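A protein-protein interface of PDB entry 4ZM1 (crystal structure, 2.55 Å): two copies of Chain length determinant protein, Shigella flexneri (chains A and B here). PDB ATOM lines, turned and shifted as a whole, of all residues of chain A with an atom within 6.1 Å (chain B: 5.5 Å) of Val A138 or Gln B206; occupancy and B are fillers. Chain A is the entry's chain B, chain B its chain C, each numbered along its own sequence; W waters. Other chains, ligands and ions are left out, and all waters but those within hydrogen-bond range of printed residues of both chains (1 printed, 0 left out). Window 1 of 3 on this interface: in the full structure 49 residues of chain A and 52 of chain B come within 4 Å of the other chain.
No position is printed for both chains.
Of chain A, only Val A138 (3.6 Å) comes within 4 Å of Gln B206.
Of the printed residues of chain B, Thr A134 touches Gln B209.
Of the printed residues of chain A, Gln B209 touches Arg A133 (3.7 Å), Thr A134 (3.7 Å) and Val A137 (3.3 Å).
Ala A139 touches none of the printed residues of chain B.
The nearest residue of chain A that does not touch Gln B206 is Thr A134 (4.7 Å).
The nearest printed residue of chain B that does not touch Glu A141 is Gln B209 (5.5 Å).
OD1 of Asn B210 lies close to O of Gln B206.
Hydrophobic or aromatic side chains of chain A within 4 Å of the printed part of chain B: Val A137 and Val A138.
Of the 10 printed residues of chain B, 5 touch a printed residue of chain A.
Printed residues of chain B that touch a printed residue of chain A: Pro B202, Tyr B205, Gln B206, Arg B208 and Gln B209.
Hydrophobic or aromatic side chains of chain B within 4 Å of the printed part of chain A: Pro B202 and Tyr B205.
Among the printed residues, Asp or Glu carboxylates within 4 Å of a Lys or Arg side-chain nitrogen of the other chain: Glu A141 with Arg B208.
The side-chain carboxylate of Glu A141 lies within salt-bridge range of the guanidinium group of Arg B208 (2.8 Å).
Water W1 lies within hydrogen-bond range of OE2 of Glu A141, O of Tyr B205 and NE of Arg B208.
Among the printed residues, pairs that only touch across the chains: Arg A133 with Gln B209, Thr A134 with Gln B209, Val A137 with Gln B209, Val A138 with Tyr B205, Val A138 with Gln B206, Glu A141 with Tyr B205 and Gln A142 with Pro B202.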
ATOM      1  N   ARG A 133     -10.525  -0.608   2.927  1.00  0.00           N
ATOM      2  CA  ARG A 133     -11.289   0.636   2.978  1.00  0.00           C
ATOM      3  C   ARG A 133     -12.005   0.718   4.321  1.00  0.00           C
ATOM      4  O   ARG A 133     -11.718   1.627   5.101  1.00  0.00           O
ATOM      5  CB  ARG A 133     -12.273   0.704   1.792  1.00  0.00           C
ATOM      6  CG  ARG A 133     -13.272   1.874   1.785  1.00  0.00           C
ATOM      7  CD  ARG A 133     -14.226   1.825   0.584  1.00  0.00           C
ATOM      8  NE  ARG A 133     -14.860   0.511   0.382  1.00  0.00           N
ATOM      9  CZ  ARG A 133     -16.009   0.120   0.932  1.00  0.00           C
ATOM     10  NH1 ARG A 133     -16.687   0.942   1.727  1.00  0.00           N
ATOM     11  NH2 ARG A 133     -16.492  -1.090   0.686  1.00  0.00           N
ATOM     12  N   THR A 134     -12.841  -0.281   4.626  1.00  0.00           N
ATOM     13  CA  THR A 134     -13.614  -0.346   5.869  1.00  0.00           C
ATOM     14  C   THR A 134     -12.698  -0.209   7.106  1.00  0.00           C
ATOM     15  O   THR A 134     -13.012   0.582   7.994  1.00  0.00           O
ATOM     16  CB  THR A 134     -14.487  -1.640   5.904  1.00  0.00           C
ATOM     17  OG1 THR A 134     -15.337  -1.670   4.748  1.00  0.00           O
ATOM     18  CG2 THR A 134     -15.392  -1.711   7.145  1.00  0.00           C
ATOM     19  N   GLN A 135     -11.552  -0.926   7.122  1.00  0.00           N
ATOM     20  CA  GLN A 135     -10.559  -0.965   8.208  1.00  0.00           C
ATOM     21  C   GLN A 135      -9.823   0.349   8.378  1.00  0.00           C
ATOM     22  O   GLN A 135      -9.439   0.684   9.498  1.00  0.00           O
ATOM     23  CB  GLN A 135      -9.549  -2.077   7.965  1.00  0.00           C
ATOM     24  CG  GLN A 135     -10.075  -3.446   8.376  1.00  0.00           C
ATOM     25  CD  GLN A 135      -9.069  -4.501   8.027  1.00  0.00           C
ATOM     26  OE1 GLN A 135      -8.945  -4.920   6.874  1.00  0.00           O
ATOM     27  NE2 GLN A 135      -8.316  -4.936   9.007  1.00  0.00           N
ATOM     28  N   GLU A 136      -9.607   1.083   7.274  1.00  0.00           N
ATOM     29  CA  GLU A 136      -8.964   2.384   7.273  1.00  0.00           C
ATOM     30  C   GLU A 136      -9.915   3.388   7.859  1.00  0.00           C
ATOM     31  O   GLU A 136      -9.472   4.208   8.676  1.00  0.00           O
ATOM     32  CB  GLU A 136      -8.537   2.799   5.867  1.00  0.00           C
ATOM     33  CG  GLU A 136      -7.204   2.205   5.447  1.00  0.00           C
ATOM     34  CD  GLU A 136      -7.063   1.918   3.966  1.00  0.00           C
ATOM     35  OE1 GLU A 136      -8.051   2.081   3.212  1.00  0.00           O
ATOM     36  OE2 GLU A 136      -5.951   1.522   3.560  1.00  0.00           O
ATOM     37  N   VAL A 137     -11.230   3.305   7.493  1.00  0.00           N
ATOM     38  CA  VAL A 137     -12.180   4.261   8.064  1.00  0.00           C
ATOM     39  C   VAL A 137     -12.229   4.055   9.591  1.00  0.00           C
ATOM     40  O   VAL A 137     -12.113   5.049  10.321  1.00  0.00           O
ATOM     41  CB  VAL A 137     -13.615   4.376   7.431  1.00  0.00           C
ATOM     42  CG1 VAL A 137     -13.604   4.192   5.912  1.00  0.00           C
ATOM     43  CG2 VAL A 137     -14.638   3.468   8.110  1.00  0.00           C
ATOM     44  N   VAL A 138     -12.311   2.783  10.079  1.00  0.00           N
ATOM     45  CA  VAL A 138     -12.415   2.632  11.533  1.00  0.00           C
ATOM     46  C   VAL A 138     -11.153   3.166  12.211  1.00  0.00           C
ATOM     47  O   VAL A 138     -11.286   3.905  13.197  1.00  0.00           O
ATOM     48  CB  VAL A 138     -12.901   1.257  12.088  1.00  0.00           C
ATOM     49  CG1 VAL A 138     -13.530   0.381  11.018  1.00  0.00           C
ATOM     50  CG2 VAL A 138     -11.867   0.519  12.910  1.00  0.00           C
ATOM     51  N   ALA A 139      -9.957   2.912  11.631  1.00  0.00           N
ATOM     52  CA  ALA A 139      -8.713   3.415  12.215  1.00  0.00           C
ATOM     53  C   ALA A 139      -8.710   4.943  12.256  1.00  0.00           C
ATOM     54  O   ALA A 139      -8.427   5.527  13.300  1.00  0.00           O
ATOM     55  CB  ALA A 139      -7.527   2.900  11.439  1.00  0.00           C
ATOM     56  N   GLN A 140      -9.116   5.587  11.147  1.00  0.00           N
ATOM     57  CA  GLN A 140      -9.222   7.042  11.026  1.00  0.00           C
ATOM     58  C   GLN A 140     -10.278   7.601  11.984  1.00  0.00           C
ATOM     59  O   GLN A 140     -10.005   8.598  12.631  1.00  0.00           O
ATOM     60  CB  GLN A 140      -9.523   7.439   9.567  1.00  0.00           C
ATOM     61  CG  GLN A 140      -9.496   8.932   9.251  1.00  0.00           C
ATOM     62  CD  GLN A 140      -8.201   9.621   9.584  1.00  0.00           C
ATOM     63  OE1 GLN A 140      -7.158   9.447   8.947  1.00  0.00           O
ATOM     64  NE2 GLN A 140      -8.259  10.437  10.615  1.00  0.00           N
ATOM     65  N   GLU A 141     -11.451   6.960  12.099  1.00  0.00           N
ATOM     66  CA  GLU A 141     -12.507   7.429  13.004  1.00  0.00           C
ATOM     67  C   GLU A 141     -12.045   7.300  14.471  1.00  0.00           C
ATOM     68  O   GLU A 141     -12.315   8.208  15.280  1.00  0.00           O
ATOM     69  CB  GLU A 141     -13.856   6.727  12.746  1.00  0.00           C
ATOM     70  CG  GLU A 141     -14.471   7.149  11.413  1.00  0.00           C
ATOM     71  CD  GLU A 141     -15.925   7.570  11.356  1.00  0.00           C
ATOM     72  OE1 GLU A 141     -16.239   8.684  11.839  1.00  0.00           O
ATOM     73  OE2 GLU A 141     -16.740   6.809  10.785  1.00  0.00           O
ATOM     74  N   GLN A 142     -11.270   6.243  14.775  1.00  0.00           N
ATOM     75  CA  GLN A 142     -10.713   6.054  16.116  1.00  0.00           C
ATOM     76  C   GLN A 142      -9.685   7.169  16.449  1.00  0.00           C
ATOM     77  O   GLN A 142      -9.737   7.750  17.539  1.00  0.00           O
ATOM     78  CB  GLN A 142     -10.084   4.657  16.256  1.00  0.00           C
ATOM     79  CG  GLN A 142     -11.104   3.536  16.490  1.00  0.00           C
ATOM     80  CD  GLN A 142     -11.212   3.093  17.945  1.00  0.00           C
ATOM     81  OE1 GLN A 142     -12.220   3.347  18.644  1.00  0.00           O
ATOM     82  NE2 GLN A 142     -10.185   2.389  18.425  1.00  0.00           N
ATOM     83  N   LYS A 143      -8.789   7.482  15.492  1.00  0.00           N
ATOM     84  CA  LYS A 143      -7.790   8.535  15.614  1.00  0.00           C
ATOM     85  C   LYS A 143      -8.471   9.895  15.845  1.00  0.00           C
ATOM     86  O   LYS A 143      -8.079  10.611  16.773  1.00  0.00           O
ATOM     87  CB  LYS A 143      -6.889   8.572  14.364  1.00  0.00           C
ATOM     88  CG  LYS A 143      -5.897   9.736  14.328  1.00  0.00           C
ATOM     89  CD  LYS A 143      -4.956   9.662  13.179  1.00  0.00           C
ATOM     90  CE  LYS A 143      -4.465  11.009  12.749  1.00  0.00           C
ATOM     91  NZ  LYS A 143      -3.508  10.893  11.617  1.00  0.00           N
ATOM     92  N   PRO B 202     -14.239   0.433  18.405  1.00  0.00           N
ATOM     93  CA  PRO B 202     -14.081   0.256  16.947  1.00  0.00           C
ATOM     94  C   PRO B 202     -15.282  -0.466  16.320  1.00  0.00           C
ATOM     95  O   PRO B 202     -15.627  -0.175  15.177  1.00  0.00           O
ATOM     96  CB  PRO B 202     -12.814  -0.600  16.815  1.00  0.00           C
ATOM     97  CG  PRO B 202     -12.074  -0.400  18.077  1.00  0.00           C
ATOM     98  CD  PRO B 202     -13.088  -0.132  19.147  1.00  0.00           C
ATOM     99  N   ASN B 203     -15.949  -1.379  17.075  1.00  0.00           N
ATOM    100  CA  ASN B 203     -17.114  -2.135  16.609  1.00  0.00           C
ATOM    101  C   ASN B 203     -18.216  -1.203  16.116  1.00  0.00           C
ATOM    102  O   ASN B 203     -18.865  -1.534  15.128  1.00  0.00           O
ATOM    103  CB  ASN B 203     -17.658  -3.039  17.707  1.00  0.00           C
ATOM    104  CG  ASN B 203     -18.773  -3.927  17.226  1.00  0.00           C
ATOM    105  OD1 ASN B 203     -19.961  -3.540  17.229  1.00  0.00           O
ATOM    106  ND2 ASN B 203     -18.406  -5.127  16.771  1.00  0.00           N
ATOM    107  N   TYR B 204     -18.423  -0.044  16.790  1.00  0.00           N
ATOM    108  CA  TYR B 204     -19.408   0.942  16.381  1.00  0.00           C
ATOM    109  C   TYR B 204     -19.068   1.491  15.011  1.00  0.00           C
ATOM    110  O   TYR B 204     -19.938   1.533  14.148  1.00  0.00           O
ATOM    111  CB  TYR B 204     -19.500   2.083  17.396  1.00  0.00           C
ATOM    112  CG  TYR B 204     -20.449   3.203  17.004  1.00  0.00           C
ATOM    113  CD1 TYR B 204     -21.807   3.122  17.286  1.00  0.00           C
ATOM    114  CD2 TYR B 204     -19.976   4.364  16.390  1.00  0.00           C
ATOM    115  CE1 TYR B 204     -22.678   4.155  16.940  1.00  0.00           C
ATOM    116  CE2 TYR B 204     -20.836   5.403  16.047  1.00  0.00           C
ATOM    117  CZ  TYR B 204     -22.185   5.287  16.313  1.00  0.00           C
ATOM    118  OH  TYR B 204     -23.012   6.303  15.951  1.00  0.00           O
ATOM    119  N   TYR B 205     -17.808   1.884  14.805  1.00  0.00           N
ATOM    120  CA  TYR B 205     -17.334   2.466  13.555  1.00  0.00           C
ATOM    121  C   TYR B 205     -17.407   1.456  12.435  1.00  0.00           C
ATOM    122  O   TYR B 205     -17.842   1.836  11.345  1.00  0.00           O
ATOM    123  CB  TYR B 205     -15.940   3.076  13.733  1.00  0.00           C
ATOM    124  CG  TYR B 205     -15.960   4.250  14.703  1.00  0.00           C
ATOM    125  CD1 TYR B 205     -16.797   5.342  14.488  1.00  0.00           C
ATOM    126  CD2 TYR B 205     -15.165   4.256  15.839  1.00  0.00           C
ATOM    127  CE1 TYR B 205     -16.834   6.417  15.374  1.00  0.00           C
ATOM    128  CE2 TYR B 205     -15.165   5.337  16.720  1.00  0.00           C
ATOM    129  CZ  TYR B 205     -16.014   6.416  16.492  1.00  0.00           C
ATOM    130  OH  TYR B 205     -16.063   7.496  17.359  1.00  0.00           O
ATOM    131  N   GLN B 206     -17.131   0.156  12.733  1.00  0.00           N
ATOM    132  CA  GLN B 206     -17.249  -0.966  11.789  1.00  0.00           C
ATOM    133  C   GLN B 206     -18.709  -1.170  11.370  1.00  0.00           C
ATOM    134  O   GLN B 206     -18.988  -1.243  10.177  1.00  0.00           O
ATOM    135  CB  GLN B 206     -16.718  -2.265  12.413  1.00  0.00           C
ATOM    136  CG  GLN B 206     -15.228  -2.328  12.633  1.00  0.00           C
ATOM    137  CD  GLN B 206     -14.804  -3.677  13.178  1.00  0.00           C
ATOM    138  OE1 GLN B 206     -15.025  -4.730  12.546  1.00  0.00           O
ATOM    139  NE2 GLN B 206     -14.170  -3.669  14.356  1.00  0.00           N
ATOM    140  N   THR B 207     -19.630  -1.257  12.368  1.00  0.00           N
ATOM    141  CA  THR B 207     -21.077  -1.439  12.212  1.00  0.00           C
ATOM    142  C   THR B 207     -21.633  -0.320  11.360  1.00  0.00           C
ATOM    143  O   THR B 207     -22.408  -0.586  10.440  1.00  0.00           O
ATOM    144  CB  THR B 207     -21.772  -1.482  13.594  1.00  0.00           C
ATOM    145  OG1 THR B 207     -21.203  -2.532  14.353  1.00  0.00           O
ATOM    146  CG2 THR B 207     -23.272  -1.711  13.514  1.00  0.00           C
ATOM    147  N   ARG B 208     -21.257   0.928  11.661  1.00  0.00           N
ATOM    148  CA  ARG B 208     -21.740   2.071  10.901  1.00  0.00           C
ATOM    149  C   ARG B 208     -21.297   1.980   9.457  1.00  0.00           C
ATOM    150  O   ARG B 208     -22.112   2.240   8.568  1.00  0.00           O
ATOM    151  CB  ARG B 208     -21.253   3.374  11.514  1.00  0.00           C
ATOM    152  CG  ARG B 208     -21.935   4.562  10.903  1.00  0.00           C
ATOM    153  CD  ARG B 208     -21.808   5.727  11.800  1.00  0.00           C
ATOM    154  NE  ARG B 208     -20.468   6.290  11.728  1.00  0.00           N
ATOM    155  CZ  ARG B 208     -20.051   7.302  12.478  1.00  0.00           C
ATOM    156  NH1 ARG B 208     -20.859   7.849  13.383  1.00  0.00           N
ATOM    157  NH2 ARG B 208     -18.827   7.768  12.341  1.00  0.00           N
ATOM    158  N   GLN B 209     -20.016   1.596   9.221  1.00  0.00           N
ATOM    159  CA  GLN B 209     -19.484   1.455   7.862  1.00  0.00           C
ATOM    160  C   GLN B 209     -20.201   0.322   7.123  1.00  0.00           C
ATOM    161  O   GLN B 209     -20.543   0.500   5.955  1.00  0.00           O
ATOM    162  CB  GLN B 209     -17.966   1.245   7.860  1.00  0.00           C
ATOM    163  CG  GLN B 209     -17.313   1.416   6.475  1.00  0.00           C
ATOM    164  CD  GLN B 209     -17.684   2.672   5.704  1.00  0.00           C
ATOM    165  OE1 GLN B 209     -18.219   2.608   4.599  1.00  0.00           O
ATOM    166  NE2 GLN B 209     -17.375   3.845   6.234  1.00  0.00           N
ATOM    167  N   ASN B 210     -20.488  -0.802   7.819  1.00  0.00           N
ATOM    168  CA  ASN B 210     -21.191  -1.939   7.236  1.00  0.00           C
ATOM    169  C   ASN B 210     -22.588  -1.541   6.791  1.00  0.00           C
ATOM    170  O   ASN B 210     -23.033  -2.032   5.742  1.00  0.00           O
ATOM    171  CB  ASN B 210     -21.281  -3.124   8.217  1.00  0.00           C
ATOM    172  CG  ASN B 210     -19.964  -3.810   8.534  1.00  0.00           C
ATOM    173  OD1 ASN B 210     -18.904  -3.583   7.886  1.00  0.00           O
ATOM    174  ND2 ASN B 210     -20.002  -4.662   9.572  1.00  0.00           N
ATOM    175  N   LEU B 211     -23.255  -0.618   7.559  1.00  0.00           N
ATOM    176  CA  LEU B 211     -24.601  -0.146   7.272  1.00  0.00           C
ATOM    177  C   LEU B 211     -24.633   0.716   6.023  1.00  0.00           C
ATOM    178  O   LEU B 211     -25.569   0.575   5.224  1.00  0.00           O
ATOM    179  CB  LEU B 211     -25.172   0.618   8.460  1.00  0.00           C
ATOM    180  CG  LEU B 211     -26.681   0.841   8.472  1.00  0.00           C
ATOM    181  CD1 LEU B 211     -27.441  -0.478   8.225  1.00  0.00           C
ATOM    182  CD2 LEU B 211     -27.107   1.454   9.754  1.00  0.00           C
HETATM  183  O   HOH W   1     -18.286   4.659  10.395  1.00  0.00           O
